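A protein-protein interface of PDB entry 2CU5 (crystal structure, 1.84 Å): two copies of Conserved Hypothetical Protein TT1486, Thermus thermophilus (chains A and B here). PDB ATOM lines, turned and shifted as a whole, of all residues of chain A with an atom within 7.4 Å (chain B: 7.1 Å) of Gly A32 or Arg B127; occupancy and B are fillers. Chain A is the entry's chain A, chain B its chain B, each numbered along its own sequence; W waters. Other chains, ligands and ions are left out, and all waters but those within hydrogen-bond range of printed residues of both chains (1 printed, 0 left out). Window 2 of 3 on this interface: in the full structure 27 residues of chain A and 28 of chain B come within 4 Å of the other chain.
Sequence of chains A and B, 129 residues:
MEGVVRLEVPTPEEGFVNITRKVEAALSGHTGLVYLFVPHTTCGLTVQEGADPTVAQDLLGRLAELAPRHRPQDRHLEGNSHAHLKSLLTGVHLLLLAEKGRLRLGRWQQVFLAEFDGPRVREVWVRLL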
ATOM      1  N   LEU A  27      13.375  -8.296  29.399  1.00  0.00           N
ATOM      2  CA  LEU A  27      13.786  -9.430  28.578  1.00  0.00           C
ATOM      3  C   LEU A  27      15.067 -10.150  28.988  1.00  0.00           C
ATOM      4  O   LEU A  27      15.295 -11.286  28.567  1.00  0.00           O
ATOM      5  CB  LEU A  27      13.918  -8.990  27.121  1.00  0.00           C
ATOM      6  CG  LEU A  27      12.652  -8.371  26.527  1.00  0.00           C
ATOM      7  CD1 LEU A  27      12.895  -8.008  25.071  1.00  0.00           C
ATOM      8  CD2 LEU A  27      11.499  -9.355  26.654  1.00  0.00           C
ATOM      9  N   GLY A  29      18.100  -9.908  27.980  1.00  0.00           N
ATOM     10  CA  GLY A  29      18.846 -10.364  26.818  1.00  0.00           C
ATOM     11  C   GLY A  29      18.250 -11.525  26.036  1.00  0.00           C
ATOM     12  O   GLY A  29      18.938 -12.155  25.236  1.00  0.00           O
ATOM     13  N   HIS A  30      16.972 -11.808  26.253  1.00  0.00           N
ATOM     14  CA  HIS A  30      16.300 -12.903  25.556  1.00  0.00           C
ATOM     15  C   HIS A  30      16.290 -12.750  24.033  1.00  0.00           C
ATOM     16  O   HIS A  30      16.257 -11.638  23.505  1.00  0.00           O
ATOM     17  CB  HIS A  30      14.849 -13.012  26.042  1.00  0.00           C
ATOM     18  CG  HIS A  30      14.019 -14.003  25.278  1.00  0.00           C
ATOM     19  ND1 HIS A  30      14.200 -15.366  25.383  1.00  0.00           N
ATOM     20  CD2 HIS A  30      13.001 -13.826  24.401  1.00  0.00           C
ATOM     21  CE1 HIS A  30      13.329 -15.985  24.604  1.00  0.00           C
ATOM     22  NE2 HIS A  30      12.590 -15.074  23.998  1.00  0.00           N
ATOM     23  N   THR A  31      16.337 -13.885  23.341  1.00  0.00           N
ATOM     24  CA  THR A  31      16.261 -13.918  21.885  1.00  0.00           C
ATOM     25  C   THR A  31      15.112 -14.862  21.550  1.00  0.00           C
ATOM     26  O   THR A  31      15.142 -16.039  21.901  1.00  0.00           O
ATOM     27  CB  THR A  31      17.548 -14.454  21.230  1.00  0.00           C
ATOM     28  OG1 THR A  31      18.595 -13.490  21.373  1.00  0.00           O
ATOM     29  CG2 THR A  31      17.317 -14.721  19.744  1.00  0.00           C
ATOM     30  N   GLY A  32      14.091 -14.334  20.883  1.00  0.00           N
ATOM     31  CA  GLY A  32      12.938 -15.144  20.528  1.00  0.00           C
ATOM     32  C   GLY A  32      11.676 -14.310  20.644  1.00  0.00           C
ATOM     33  O   GLY A  32      11.751 -13.101  20.859  1.00  0.00           O
ATOM     34  N   LEU A  33      10.518 -14.944  20.513  1.00  0.00           N
ATOM     35  CA  LEU A  33       9.260 -14.217  20.608  1.00  0.00           C
ATOM     36  C   LEU A  33       8.981 -13.768  22.038  1.00  0.00           C
ATOM     37  O   LEU A  33       9.421 -14.397  23.001  1.00  0.00           O
ATOM     38  CB  LEU A  33       8.110 -15.084  20.084  1.00  0.00           C
ATOM     39  CG  LEU A  33       8.128 -15.262  18.563  1.00  0.00           C
ATOM     40  CD1 LEU A  33       7.167 -16.354  18.130  1.00  0.00           C
ATOM     41  CD2 LEU A  33       7.771 -13.934  17.914  1.00  0.00           C
ATOM     42  N   VAL A  34       8.257 -12.660  22.156  1.00  0.00           N
ATOM     43  CA  VAL A  34       7.892 -12.080  23.441  1.00  0.00           C
ATOM     44  C   VAL A  34       6.386 -11.834  23.451  1.00  0.00           C
ATOM     45  O   VAL A  34       5.846 -11.229  22.525  1.00  0.00           O
ATOM     46  CB  VAL A  34       8.610 -10.728  23.669  1.00  0.00           C
ATOM     47  CG1 VAL A  34       8.140 -10.101  24.970  1.00  0.00           C
ATOM     48  CG2 VAL A  34      10.127 -10.932  23.687  1.00  0.00           C
ATOM     49  N   TYR A  35       5.718 -12.309  24.494  1.00  0.00           N
ATOM     50  CA  TYR A  35       4.274 -12.135  24.630  1.00  0.00           C
ATOM     51  C   TYR A  35       3.984 -10.996  25.609  1.00  0.00           C
ATOM     52  O   TYR A  35       4.608 -10.910  26.670  1.00  0.00           O
ATOM     53  CB  TYR A  35       3.641 -13.436  25.137  1.00  0.00           C
ATOM     54  CG  TYR A  35       2.179 -13.332  25.508  1.00  0.00           C
ATOM     55  CD1 TYR A  35       1.193 -13.200  24.529  1.00  0.00           C
ATOM     56  CD2 TYR A  35       1.781 -13.358  26.843  1.00  0.00           C
ATOM     57  CE1 TYR A  35      -0.162 -13.097  24.879  1.00  0.00           C
ATOM     58  CE2 TYR A  35       0.433 -13.259  27.201  1.00  0.00           C
ATOM     59  CZ  TYR A  35      -0.531 -13.129  26.215  1.00  0.00           C
ATOM     60  OH  TYR A  35      -1.857 -13.038  26.577  1.00  0.00           O
ATOM     61  N   LEU A  96       5.788 -10.199  19.843  1.00  0.00           N
ATOM     62  CA  LEU A  96       6.874  -9.557  19.116  1.00  0.00           C
ATOM     63  C   LEU A  96       8.189 -10.326  19.169  1.00  0.00           C
ATOM     64  O   LEU A  96       8.424 -11.118  20.080  1.00  0.00           O
ATOM     65  CB  LEU A  96       7.097  -8.155  19.690  1.00  0.00           C
ATOM     66  CG  LEU A  96       5.868  -7.235  19.716  1.00  0.00           C
ATOM     67  CD1 LEU A  96       6.047  -6.143  20.758  1.00  0.00           C
ATOM     68  CD2 LEU A  96       5.652  -6.643  18.328  1.00  0.00           C
ATOM     69  N   LEU A  97       9.039 -10.066  18.181  1.00  0.00           N
ATOM     70  CA  LEU A  97      10.355 -10.694  18.078  1.00  0.00           C
ATOM     71  C   LEU A  97      11.377  -9.886  18.865  1.00  0.00           C
ATOM     72  O   LEU A  97      11.341  -8.655  18.864  1.00  0.00           O
ATOM     73  CB  LEU A  97      10.808 -10.735  16.620  1.00  0.00           C
ATOM     74  CG  LEU A  97       9.994 -11.558  15.630  1.00  0.00           C
ATOM     75  CD1 LEU A  97      10.388 -11.186  14.201  1.00  0.00           C
ATOM     76  CD2 LEU A  97      10.230 -13.025  15.895  1.00  0.00           C
ATOM     77  N   ALA A  98      12.290 -10.584  19.529  1.00  0.00           N
ATOM     78  CA  ALA A  98      13.339  -9.933  20.293  1.00  0.00           C
ATOM     79  C   ALA A  98      14.668 -10.596  19.956  1.00  0.00           C
ATOM     80  O   ALA A  98      14.725 -11.792  19.679  1.00  0.00           O
ATOM     81  CB  ALA A  98      13.062 -10.052  21.791  1.00  0.00           C
ATOM     82  N   GLU A  99      15.732  -9.807  19.960  1.00  0.00           N
ATOM     83  CA  GLU A  99      17.059 -10.330  19.683  1.00  0.00           C
ATOM     84  C   GLU A  99      18.008  -9.774  20.728  1.00  0.00           C
ATOM     85  O   GLU A  99      18.242  -8.568  20.790  1.00  0.00           O
ATOM     86  CB  GLU A  99      17.520  -9.921  18.286  1.00  0.00           C
ATOM     87  CG  GLU A  99      18.921 -10.403  17.939  1.00  0.00           C
ATOM     88  CD  GLU A  99      19.315 -10.062  16.517  1.00  0.00           C
ATOM     89  OE1 GLU A  99      18.698 -10.613  15.579  1.00  0.00           O
ATOM     90  OE2 GLU A  99      20.237  -9.238  16.332  1.00  0.00           O
ATOM     91  N   LYS A 100      18.532 -10.665  21.562  1.00  0.00           N
ATOM     92  CA  LYS A 100      19.459 -10.284  22.614  1.00  0.00           C
ATOM     93  C   LYS A 100      18.945  -9.137  23.482  1.00  0.00           C
ATOM     94  O   LYS A 100      19.655  -8.165  23.745  1.00  0.00           O
ATOM     95  CB  LYS A 100      20.814  -9.938  21.991  1.00  0.00           C
ATOM     96  CG  LYS A 100      21.410 -11.119  21.229  1.00  0.00           C
ATOM     97  CD  LYS A 100      22.675 -10.767  20.462  1.00  0.00           C
ATOM     98  CE  LYS A 100      23.182 -11.982  19.688  1.00  0.00           C
ATOM     99  NZ  LYS A 100      24.382 -11.681  18.857  1.00  0.00           N
ATOM    100  N   GLY A 101      17.698  -9.261  23.926  1.00  0.00           N
ATOM    101  CA  GLY A 101      17.109  -8.254  24.789  1.00  0.00           C
ATOM    102  C   GLY A 101      16.511  -7.039  24.115  1.00  0.00           C
ATOM    103  O   GLY A 101      16.007  -6.150  24.797  1.00  0.00           O
ATOM    104  N   ARG A 102      16.564  -6.984  22.789  1.00  0.00           N
ATOM    105  CA  ARG A 102      16.003  -5.848  22.073  1.00  0.00           C
ATOM    106  C   ARG A 102      14.911  -6.267  21.102  1.00  0.00           C
ATOM    107  O   ARG A 102      15.071  -7.213  20.334  1.00  0.00           O
ATOM    108  CB  ARG A 102      17.109  -5.090  21.336  1.00  0.00           C
ATOM    109  CG  ARG A 102      18.085  -4.398  22.286  1.00  0.00           C
ATOM    110  CD  ARG A 102      19.130  -3.586  21.543  1.00  0.00           C
ATOM    111  NE  ARG A 102      20.046  -2.907  22.458  1.00  0.00           N
ATOM    112  CZ  ARG A 102      20.878  -3.528  23.293  1.00  0.00           C
ATOM    113  NH1 ARG A 102      20.919  -4.854  23.339  1.00  0.00           N
ATOM    114  NH2 ARG A 102      21.674  -2.820  24.082  1.00  0.00           N
ATOM    115  N   LEU A 103      13.793  -5.552  21.147  1.00  0.00           N
ATOM    116  CA  LEU A 103      12.668  -5.844  20.273  1.00  0.00           C
ATOM    117  C   LEU A 103      13.013  -5.522  18.824  1.00  0.00           C
ATOM    118  O   LEU A 103      13.596  -4.478  18.540  1.00  0.00           O
ATOM    119  CB  LEU A 103      11.450  -5.034  20.716  1.00  0.00           C
ATOM    120  CG  LEU A 103      10.886  -5.418  22.088  1.00  0.00           C
ATOM    121  CD1 LEU A 103       9.887  -4.360  22.565  1.00  0.00           C
ATOM    122  CD2 LEU A 103      10.236  -6.784  21.995  1.00  0.00           C
ATOM    123  N   ARG A 104      12.663  -6.431  17.915  1.00  0.00           N
ATOM    124  CA  ARG A 104      12.914  -6.242  16.486  1.00  0.00           C
ATOM    125  C   ARG A 104      11.683  -5.561  15.904  1.00  0.00           C
ATOM    126  O   ARG A 104      10.628  -6.178  15.765  1.00  0.00           O
ATOM    127  CB  ARG A 104      13.135  -7.588  15.791  1.00  0.00           C
ATOM    128  CG  ARG A 104      14.275  -8.410  16.364  1.00  0.00           C
ATOM    129  CD  ARG A 104      15.619  -7.689  16.277  1.00  0.00           C
ATOM    130  NE  ARG A 104      16.128  -7.552  14.910  1.00  0.00           N
ATOM    131  CZ  ARG A 104      15.816  -6.563  14.075  1.00  0.00           C
ATOM    132  NH1 ARG A 104      14.987  -5.597  14.451  1.00  0.00           N
ATOM    133  NH2 ARG A 104      16.345  -6.534  12.857  1.00  0.00           N
ATOM    134  N   LEU A 128       8.326 -14.668  27.891  1.00  0.00           N
ATOM    135  CA  LEU A 128       9.285 -15.014  26.850  1.00  0.00           C
ATOM    136  C   LEU A 128       8.967 -16.420  26.352  1.00  0.00           C
ATOM    137  O   LEU A 128       8.754 -17.330  27.151  1.00  0.00           O
ATOM    138  CB  LEU A 128      10.713 -14.989  27.410  1.00  0.00           C
ATOM    139  CG  LEU A 128      11.098 -13.794  28.292  1.00  0.00           C
ATOM    140  CD1 LEU A 128      12.510 -13.980  28.832  1.00  0.00           C
ATOM    141  CD2 LEU A 128      10.999 -12.509  27.494  1.00  0.00           C
ATOM    142  N   LEU A 129       8.916 -16.590  25.035  1.00  0.00           N
ATOM    143  CA  LEU A 129       8.657 -17.899  24.449  1.00  0.00           C
ATOM    144  C   LEU A 129       9.999 -18.514  24.065  1.00  0.00           C
ATOM    145  O   LEU A 129      10.949 -17.741  23.811  1.00  0.00           O
ATOM    146  CB  LEU A 129       7.791 -17.787  23.189  1.00  0.00           C
ATOM    147  CG  LEU A 129       6.305 -17.448  23.326  1.00  0.00           C
ATOM    148  CD1 LEU A 129       6.133 -16.025  23.841  1.00  0.00           C
ATOM    149  CD2 LEU A 129       5.637 -17.615  21.972  1.00  0.00           C
ATOM    150  OXT LEU A 129      10.074 -19.755  23.995  1.00  0.00           O
ATOM    151  N   GLY B   3      16.675 -15.583  12.158  1.00  0.00           N
ATOM    152  CA  GLY B   3      15.658 -16.554  12.660  1.00  0.00           C
ATOM    153  C   GLY B   3      14.282 -16.351  12.051  1.00  0.00           C
ATOM    154  O   GLY B   3      13.321 -17.026  12.423  1.00  0.00           O
ATOM    155  N   VAL B   4      14.179 -15.418  11.112  1.00  0.00           N
ATOM    156  CA  VAL B   4      12.904 -15.147  10.461  1.00  0.00           C
ATOM    157  C   VAL B   4      13.061 -15.066   8.948  1.00  0.00           C
ATOM    158  O   VAL B   4      14.115 -14.675   8.443  1.00  0.00           O
ATOM    159  CB  VAL B   4      12.291 -13.815  10.957  1.00  0.00           C
ATOM    160  CG1 VAL B   4      12.322 -13.764  12.476  1.00  0.00           C
ATOM    161  CG2 VAL B   4      13.045 -12.631  10.359  1.00  0.00           C
ATOM    162  N   VAL B   5      12.007 -15.447   8.232  1.00  0.00           N
ATOM    163  CA  VAL B   5      12.006 -15.392   6.778  1.00  0.00           C
ATOM    164  C   VAL B   5      11.239 -14.138   6.387  1.00  0.00           C
ATOM    165  O   VAL B   5      10.192 -13.843   6.964  1.00  0.00           O
ATOM    166  CB  VAL B   5      11.314 -16.628   6.166  1.00  0.00           C
ATOM    167  CG1 VAL B   5      11.206 -16.480   4.658  1.00  0.00           C
ATOM    168  CG2 VAL B   5      12.107 -17.882   6.506  1.00  0.00           C
ATOM    169  N   LEU B  27       6.995 -21.914   4.123  1.00  0.00           N
ATOM    170  CA  LEU B  27       6.878 -22.905   5.188  1.00  0.00           C
ATOM    171  C   LEU B  27       7.549 -24.230   4.832  1.00  0.00           C
ATOM    172  O   LEU B  27       7.950 -24.989   5.714  1.00  0.00           O
ATOM    173  CB  LEU B  27       5.404 -23.171   5.505  1.00  0.00           C
ATOM    174  CG  LEU B  27       4.574 -22.018   6.075  1.00  0.00           C
ATOM    175  CD1 LEU B  27       3.197 -22.542   6.449  1.00  0.00           C
ATOM    176  CD2 LEU B  27       5.270 -21.436   7.298  1.00  0.00           C
ATOM    177  N   HIS B  30       6.225 -27.148   6.775  1.00  0.00           N
ATOM    178  CA  HIS B  30       6.222 -27.030   8.228  1.00  0.00           C
ATOM    179  C   HIS B  30       4.882 -27.312   8.907  1.00  0.00           C
ATOM    180  O   HIS B  30       3.819 -27.001   8.370  1.00  0.00           O
ATOM    181  CB  HIS B  30       6.684 -25.631   8.641  1.00  0.00           C
ATOM    182  CG  HIS B  30       6.916 -25.483  10.116  1.00  0.00           C
ATOM    183  ND1 HIS B  30       7.926 -26.147  10.780  1.00  0.00           N
ATOM    184  CD2 HIS B  30       6.270 -24.748  11.052  1.00  0.00           C
ATOM    185  CE1 HIS B  30       7.892 -25.826  12.061  1.00  0.00           C
ATOM    186  NE2 HIS B  30       6.896 -24.978  12.254  1.00  0.00           N
ATOM    187  N   LEU B  33       2.814 -23.791  14.881  1.00  0.00           N
ATOM    188  CA  LEU B  33       2.366 -22.404  14.842  1.00  0.00           C
ATOM    189  C   LEU B  33       3.334 -21.522  14.060  1.00  0.00           C
ATOM    190  O   LEU B  33       4.554 -21.698  14.126  1.00  0.00           O
ATOM    191  CB  LEU B  33       2.188 -21.867  16.266  1.00  0.00           C
ATOM    192  CG  LEU B  33       0.955 -22.411  16.997  1.00  0.00           C
ATOM    193  CD1 LEU B  33       0.996 -22.016  18.463  1.00  0.00           C
ATOM    194  CD2 LEU B  33      -0.310 -21.869  16.328  1.00  0.00           C
ATOM    195  N   VAL B  34       2.772 -20.567  13.320  1.00  0.00           N
ATOM    196  CA  VAL B  34       3.541 -19.653  12.493  1.00  0.00           C
ATOM    197  C   VAL B  34       3.235 -18.200  12.852  1.00  0.00           C
ATOM    198  O   VAL B  34       2.075 -17.806  12.896  1.00  0.00           O
ATOM    199  CB  VAL B  34       3.205 -19.866  10.997  1.00  0.00           C
ATOM    200  CG1 VAL B  34       4.005 -18.909  10.139  1.00  0.00           C
ATOM    201  CG2 VAL B  34       3.479 -21.309  10.596  1.00  0.00           C
ATOM    202  N   TYR B  35       4.279 -17.409  13.090  1.00  0.00           N
ATOM    203  CA  TYR B  35       4.134 -15.994  13.440  1.00  0.00           C
ATOM    204  C   TYR B  35       4.376 -15.088  12.230  1.00  0.00           C
ATOM    205  O   TYR B  35       5.354 -15.258  11.501  1.00  0.00           O
ATOM    206  CB  TYR B  35       5.125 -15.637  14.557  1.00  0.00           C
ATOM    207  CG  TYR B  35       5.254 -14.158  14.874  1.00  0.00           C
ATOM    208  CD1 TYR B  35       4.286 -13.496  15.632  1.00  0.00           C
ATOM    209  CD2 TYR B  35       6.365 -13.434  14.455  1.00  0.00           C
ATOM    210  CE1 TYR B  35       4.434 -12.150  15.970  1.00  0.00           C
ATOM    211  CE2 TYR B  35       6.521 -12.089  14.783  1.00  0.00           C
ATOM    212  CZ  TYR B  35       5.558 -11.455  15.544  1.00  0.00           C
ATOM    213  OH  TYR B  35       5.743 -10.142  15.909  1.00  0.00           O
ATOM    214  N   LEU B  36       3.473 -14.128  12.027  1.00  0.00           N
ATOM    215  CA  LEU B  36       3.569 -13.176  10.923  1.00  0.00           C
ATOM    216  C   LEU B  36       3.524 -11.759  11.492  1.00  0.00           C
ATOM    217  O   LEU B  36       2.730 -11.470  12.392  1.00  0.00           O
ATOM    218  CB  LEU B  36       2.411 -13.386   9.942  1.00  0.00           C
ATOM    219  CG  LEU B  36       2.287 -14.790   9.339  1.00  0.00           C
ATOM    220  CD1 LEU B  36       1.048 -14.863   8.456  1.00  0.00           C
ATOM    221  CD2 LEU B  36       3.542 -15.121   8.538  1.00  0.00           C
ATOM    222  N   PHE B  37       4.356 -10.876  10.954  1.00  0.00           N
ATOM    223  CA  PHE B  37       4.434  -9.507  11.454  1.00  0.00           C
ATOM    224  C   PHE B  37       4.811  -8.516  10.353  1.00  0.00           C
ATOM    225  O   PHE B  37       5.668  -8.803   9.525  1.00  0.00           O
ATOM    226  CB  PHE B  37       5.487  -9.477  12.573  1.00  0.00           C
ATOM    227  CG  PHE B  37       5.753  -8.113  13.149  1.00  0.00           C
ATOM    228  CD1 PHE B  37       4.885  -7.553  14.082  1.00  0.00           C
ATOM    229  CD2 PHE B  37       6.899  -7.408  12.791  1.00  0.00           C
ATOM    230  CE1 PHE B  37       5.157  -6.313  14.652  1.00  0.00           C
ATOM    231  CE2 PHE B  37       7.180  -6.165  13.356  1.00  0.00           C
ATOM    232  CZ  PHE B  37       6.307  -5.617  14.291  1.00  0.00           C
ATOM    233  N   LEU B  95      -0.912 -15.074  14.380  1.00  0.00           N
ATOM    234  CA  LEU B  95      -0.364 -16.330  14.869  1.00  0.00           C
ATOM    235  C   LEU B  95      -1.324 -17.343  14.273  1.00  0.00           C
ATOM    236  O   LEU B  95      -2.517 -17.326  14.572  1.00  0.00           O
ATOM    237  CB  LEU B  95      -0.370 -16.391  16.400  1.00  0.00           C
ATOM    238  CG  LEU B  95       0.293 -17.648  16.985  1.00  0.00           C
ATOM    239  CD1 LEU B  95       1.705 -17.794  16.445  1.00  0.00           C
ATOM    240  CD2 LEU B  95       0.307 -17.560  18.506  1.00  0.00           C
ATOM    241  N   TRP B 125       7.359 -10.488   8.039  1.00  0.00           N
ATOM    242  CA  TRP B 125       8.296 -11.370   8.715  1.00  0.00           C
ATOM    243  C   TRP B 125       7.578 -12.647   9.114  1.00  0.00           C
ATOM    244  O   TRP B 125       6.466 -12.615   9.649  1.00  0.00           O
ATOM    245  CB  TRP B 125       8.892 -10.681   9.945  1.00  0.00           C
ATOM    246  CG  TRP B 125       9.672  -9.441   9.621  1.00  0.00           C
ATOM    247  CD1 TRP B 125      10.062  -9.014   8.381  1.00  0.00           C
ATOM    248  CD2 TRP B 125      10.187  -8.483  10.553  1.00  0.00           C
ATOM    249  NE1 TRP B 125      10.788  -7.854   8.484  1.00  0.00           N
ATOM    250  CE2 TRP B 125      10.881  -7.505   9.805  1.00  0.00           C
ATOM    251  CE3 TRP B 125      10.132  -8.356  11.947  1.00  0.00           C
ATOM    252  CZ2 TRP B 125      11.516  -6.411  10.408  1.00  0.00           C
ATOM    253  CZ3 TRP B 125      10.763  -7.270  12.548  1.00  0.00           C
ATOM    254  CH2 TRP B 125      11.445  -6.311  11.777  1.00  0.00           C
ATOM    255  N   VAL B 126       8.220 -13.776   8.836  1.00  0.00           N
ATOM    256  CA  VAL B 126       7.660 -15.080   9.144  1.00  0.00           C
ATOM    257  C   VAL B 126       8.597 -15.820  10.099  1.00  0.00           C
ATOM    258  O   VAL B 126       9.807 -15.877   9.874  1.00  0.00           O
ATOM    259  CB  VAL B 126       7.502 -15.932   7.859  1.00  0.00           C
ATOM    260  CG1 VAL B 126       6.859 -17.265   8.190  1.00  0.00           C
ATOM    261  CG2 VAL B 126       6.670 -15.179   6.820  1.00  0.00           C
ATOM    262  N   ARG B 127       8.041 -16.372  11.169  1.00  0.00           N
ATOM    263  CA  ARG B 127       8.848 -17.125  12.119  1.00  0.00           C
ATOM    264  C   ARG B 127       8.117 -18.370  12.583  1.00  0.00           C
ATOM    265  O   ARG B 127       6.936 -18.320  12.938  1.00  0.00           O
ATOM    266  CB  ARG B 127       9.210 -16.279  13.338  1.00  0.00           C
ATOM    267  CG  ARG B 127      10.166 -16.998  14.296  1.00  0.00           C
ATOM    268  CD  ARG B 127      10.322 -16.240  15.596  1.00  0.00           C
ATOM    269  NE  ARG B 127      11.172 -16.932  16.565  1.00  0.00           N
ATOM    270  CZ  ARG B 127      12.497 -16.994  16.499  1.00  0.00           C
ATOM    271  NH1 ARG B 127      13.150 -16.409  15.503  1.00  0.00           N
ATOM    272  NH2 ARG B 127      13.175 -17.620  17.451  1.00  0.00           N
ATOM    273  N   LEU B 128       8.823 -19.493  12.567  1.00  0.00           N
ATOM    274  CA  LEU B 128       8.252 -20.754  13.004  1.00  0.00           C
ATOM    275  C   LEU B 128       8.514 -20.868  14.503  1.00  0.00           C
ATOM    276  O   LEU B 128       9.661 -20.773  14.939  1.00  0.00           O
ATOM    277  CB  LEU B 128       8.924 -21.914  12.266  1.00  0.00           C
ATOM    278  CG  LEU B 128       9.028 -21.742  10.748  1.00  0.00           C
ATOM    279  CD1 LEU B 128       9.700 -22.961  10.145  1.00  0.00           C
ATOM    280  CD2 LEU B 128       7.642 -21.543  10.144  1.00  0.00           C
ATOM    281  N   LEU B 129       7.452 -21.060  15.289  1.00  0.00           N
ATOM    282  CA  LEU B 129       7.593 -21.186  16.741  1.00  0.00           C
ATOM    283  C   LEU B 129       8.245 -22.510  17.121  1.00  0.00           C
ATOM    284  O   LEU B 129       8.126 -23.476  16.330  1.00  0.00           O
ATOM    285  CB  LEU B 129       6.225 -21.089  17.434  1.00  0.00           C
ATOM    286  CG  LEU B 129       5.680 -19.696  17.784  1.00  0.00           C
ATOM    287  CD1 LEU B 129       5.391 -18.912  16.522  1.00  0.00           C
ATOM    288  CD2 LEU B 129       4.415 -19.850  18.619  1.00  0.00           C
ATOM    289  OXT LEU B 129       8.845 -22.568  18.220  1.00  0.00           O
HETATM  290  O   HOH W   1      10.310 -18.181  19.465  1.00  0.00           O
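Of the 16 printed residues of chain B, 6 touch a printed residue of chain A.
Hydrophobic or aromatic side chains of chain B within 4 Å of the printed part of chain A: Val B4, Tyr B35, Phe B37, Trp B125 and Leu B129.
Printed residues of chain A that touch a printed residue of chain B: Gly A32, Leu A33, Leu A96, Leu A97 and Arg A104.
Hydrophobic or aromatic side chains of chain A that line the printed part of chain B: Leu A33, Leu A96 and Leu A97.
Among the printed residues, no Asp or Glu carboxylate lies within 4 Å of a Lys or Arg side-chain nitrogen of the other chain.
Of chain B, only Arg B127 (3.96 Å) comes within 4 Å of Gly A32.
Printed residues of chain B within 4 Å of Arg A104: Trp B125.
Leu A128 touches none of the printed residues of chain B.
Of the printed residues of chain A, Tyr B35 touches Leu A33 (3.8 Å), Leu A96 (3.5 Å) and Leu A97 (3.6 Å).
Printed residues of chain A within 4 Å of Arg B127: Gly A32, Leu A33 and Leu A97.
Leu A33 touches Tyr B35, but with the chains exchanged Tyr A35 does not touch Leu B33 (10.7 Å).
Leu A33 touches Leu B129, but with the chains exchanged Leu A129 does not touch Leu B33 (7.3 Å).
Among the printed residues, pairs that only touch across the chains: Leu A97 with Arg B127 (3.2 Å), Arg A104 with Trp B125 (3.4 Å), Leu A96 with Tyr B35 (3.5 Å), Leu A33 with Leu B129 (3.5 Å), Leu A97 with Tyr B35 (3.6 Å), Leu A97 with Trp B125 (3.6 Å), Leu A97 with Val B4 (3.7 Å), Leu A96 with Phe B37 (3.7 Å), Leu A33 with Tyr B35 (3.8 Å), Leu A33 with Arg B127 (3.8 Å) and Gly A32 with Arg B127 (3.96 Å).
O of Leu A33 is in hydrogen-bond range of N of Leu A129.
O of Arg B127 is in hydrogen-bond range of N of Tyr B35, at 2.8 Å.
The backbone carbonyl oxygen (O) of Leu B33 is in hydrogen-bond range of the backbone NH (N) of Leu B129 (3.2 Å).
The backbone carbonyl oxygen of Ala A98 sits at hydrogen-bond distance from the backbone NH of Gly A32 (2.9 Å).
The backbone carbonyl oxygen of Gly B3 is in hydrogen-bond range of the guanidinium group of Arg B127, at 3.1 Å.
The backbone NH (N) of Val A34 is in hydrogen-bond range of the backbone carbonyl oxygen (O) of Leu A96 (2.6 Å).
Water W1 bridges NE of Arg B127 (3.3 Å) and N of Leu A33 (3.4 Å).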
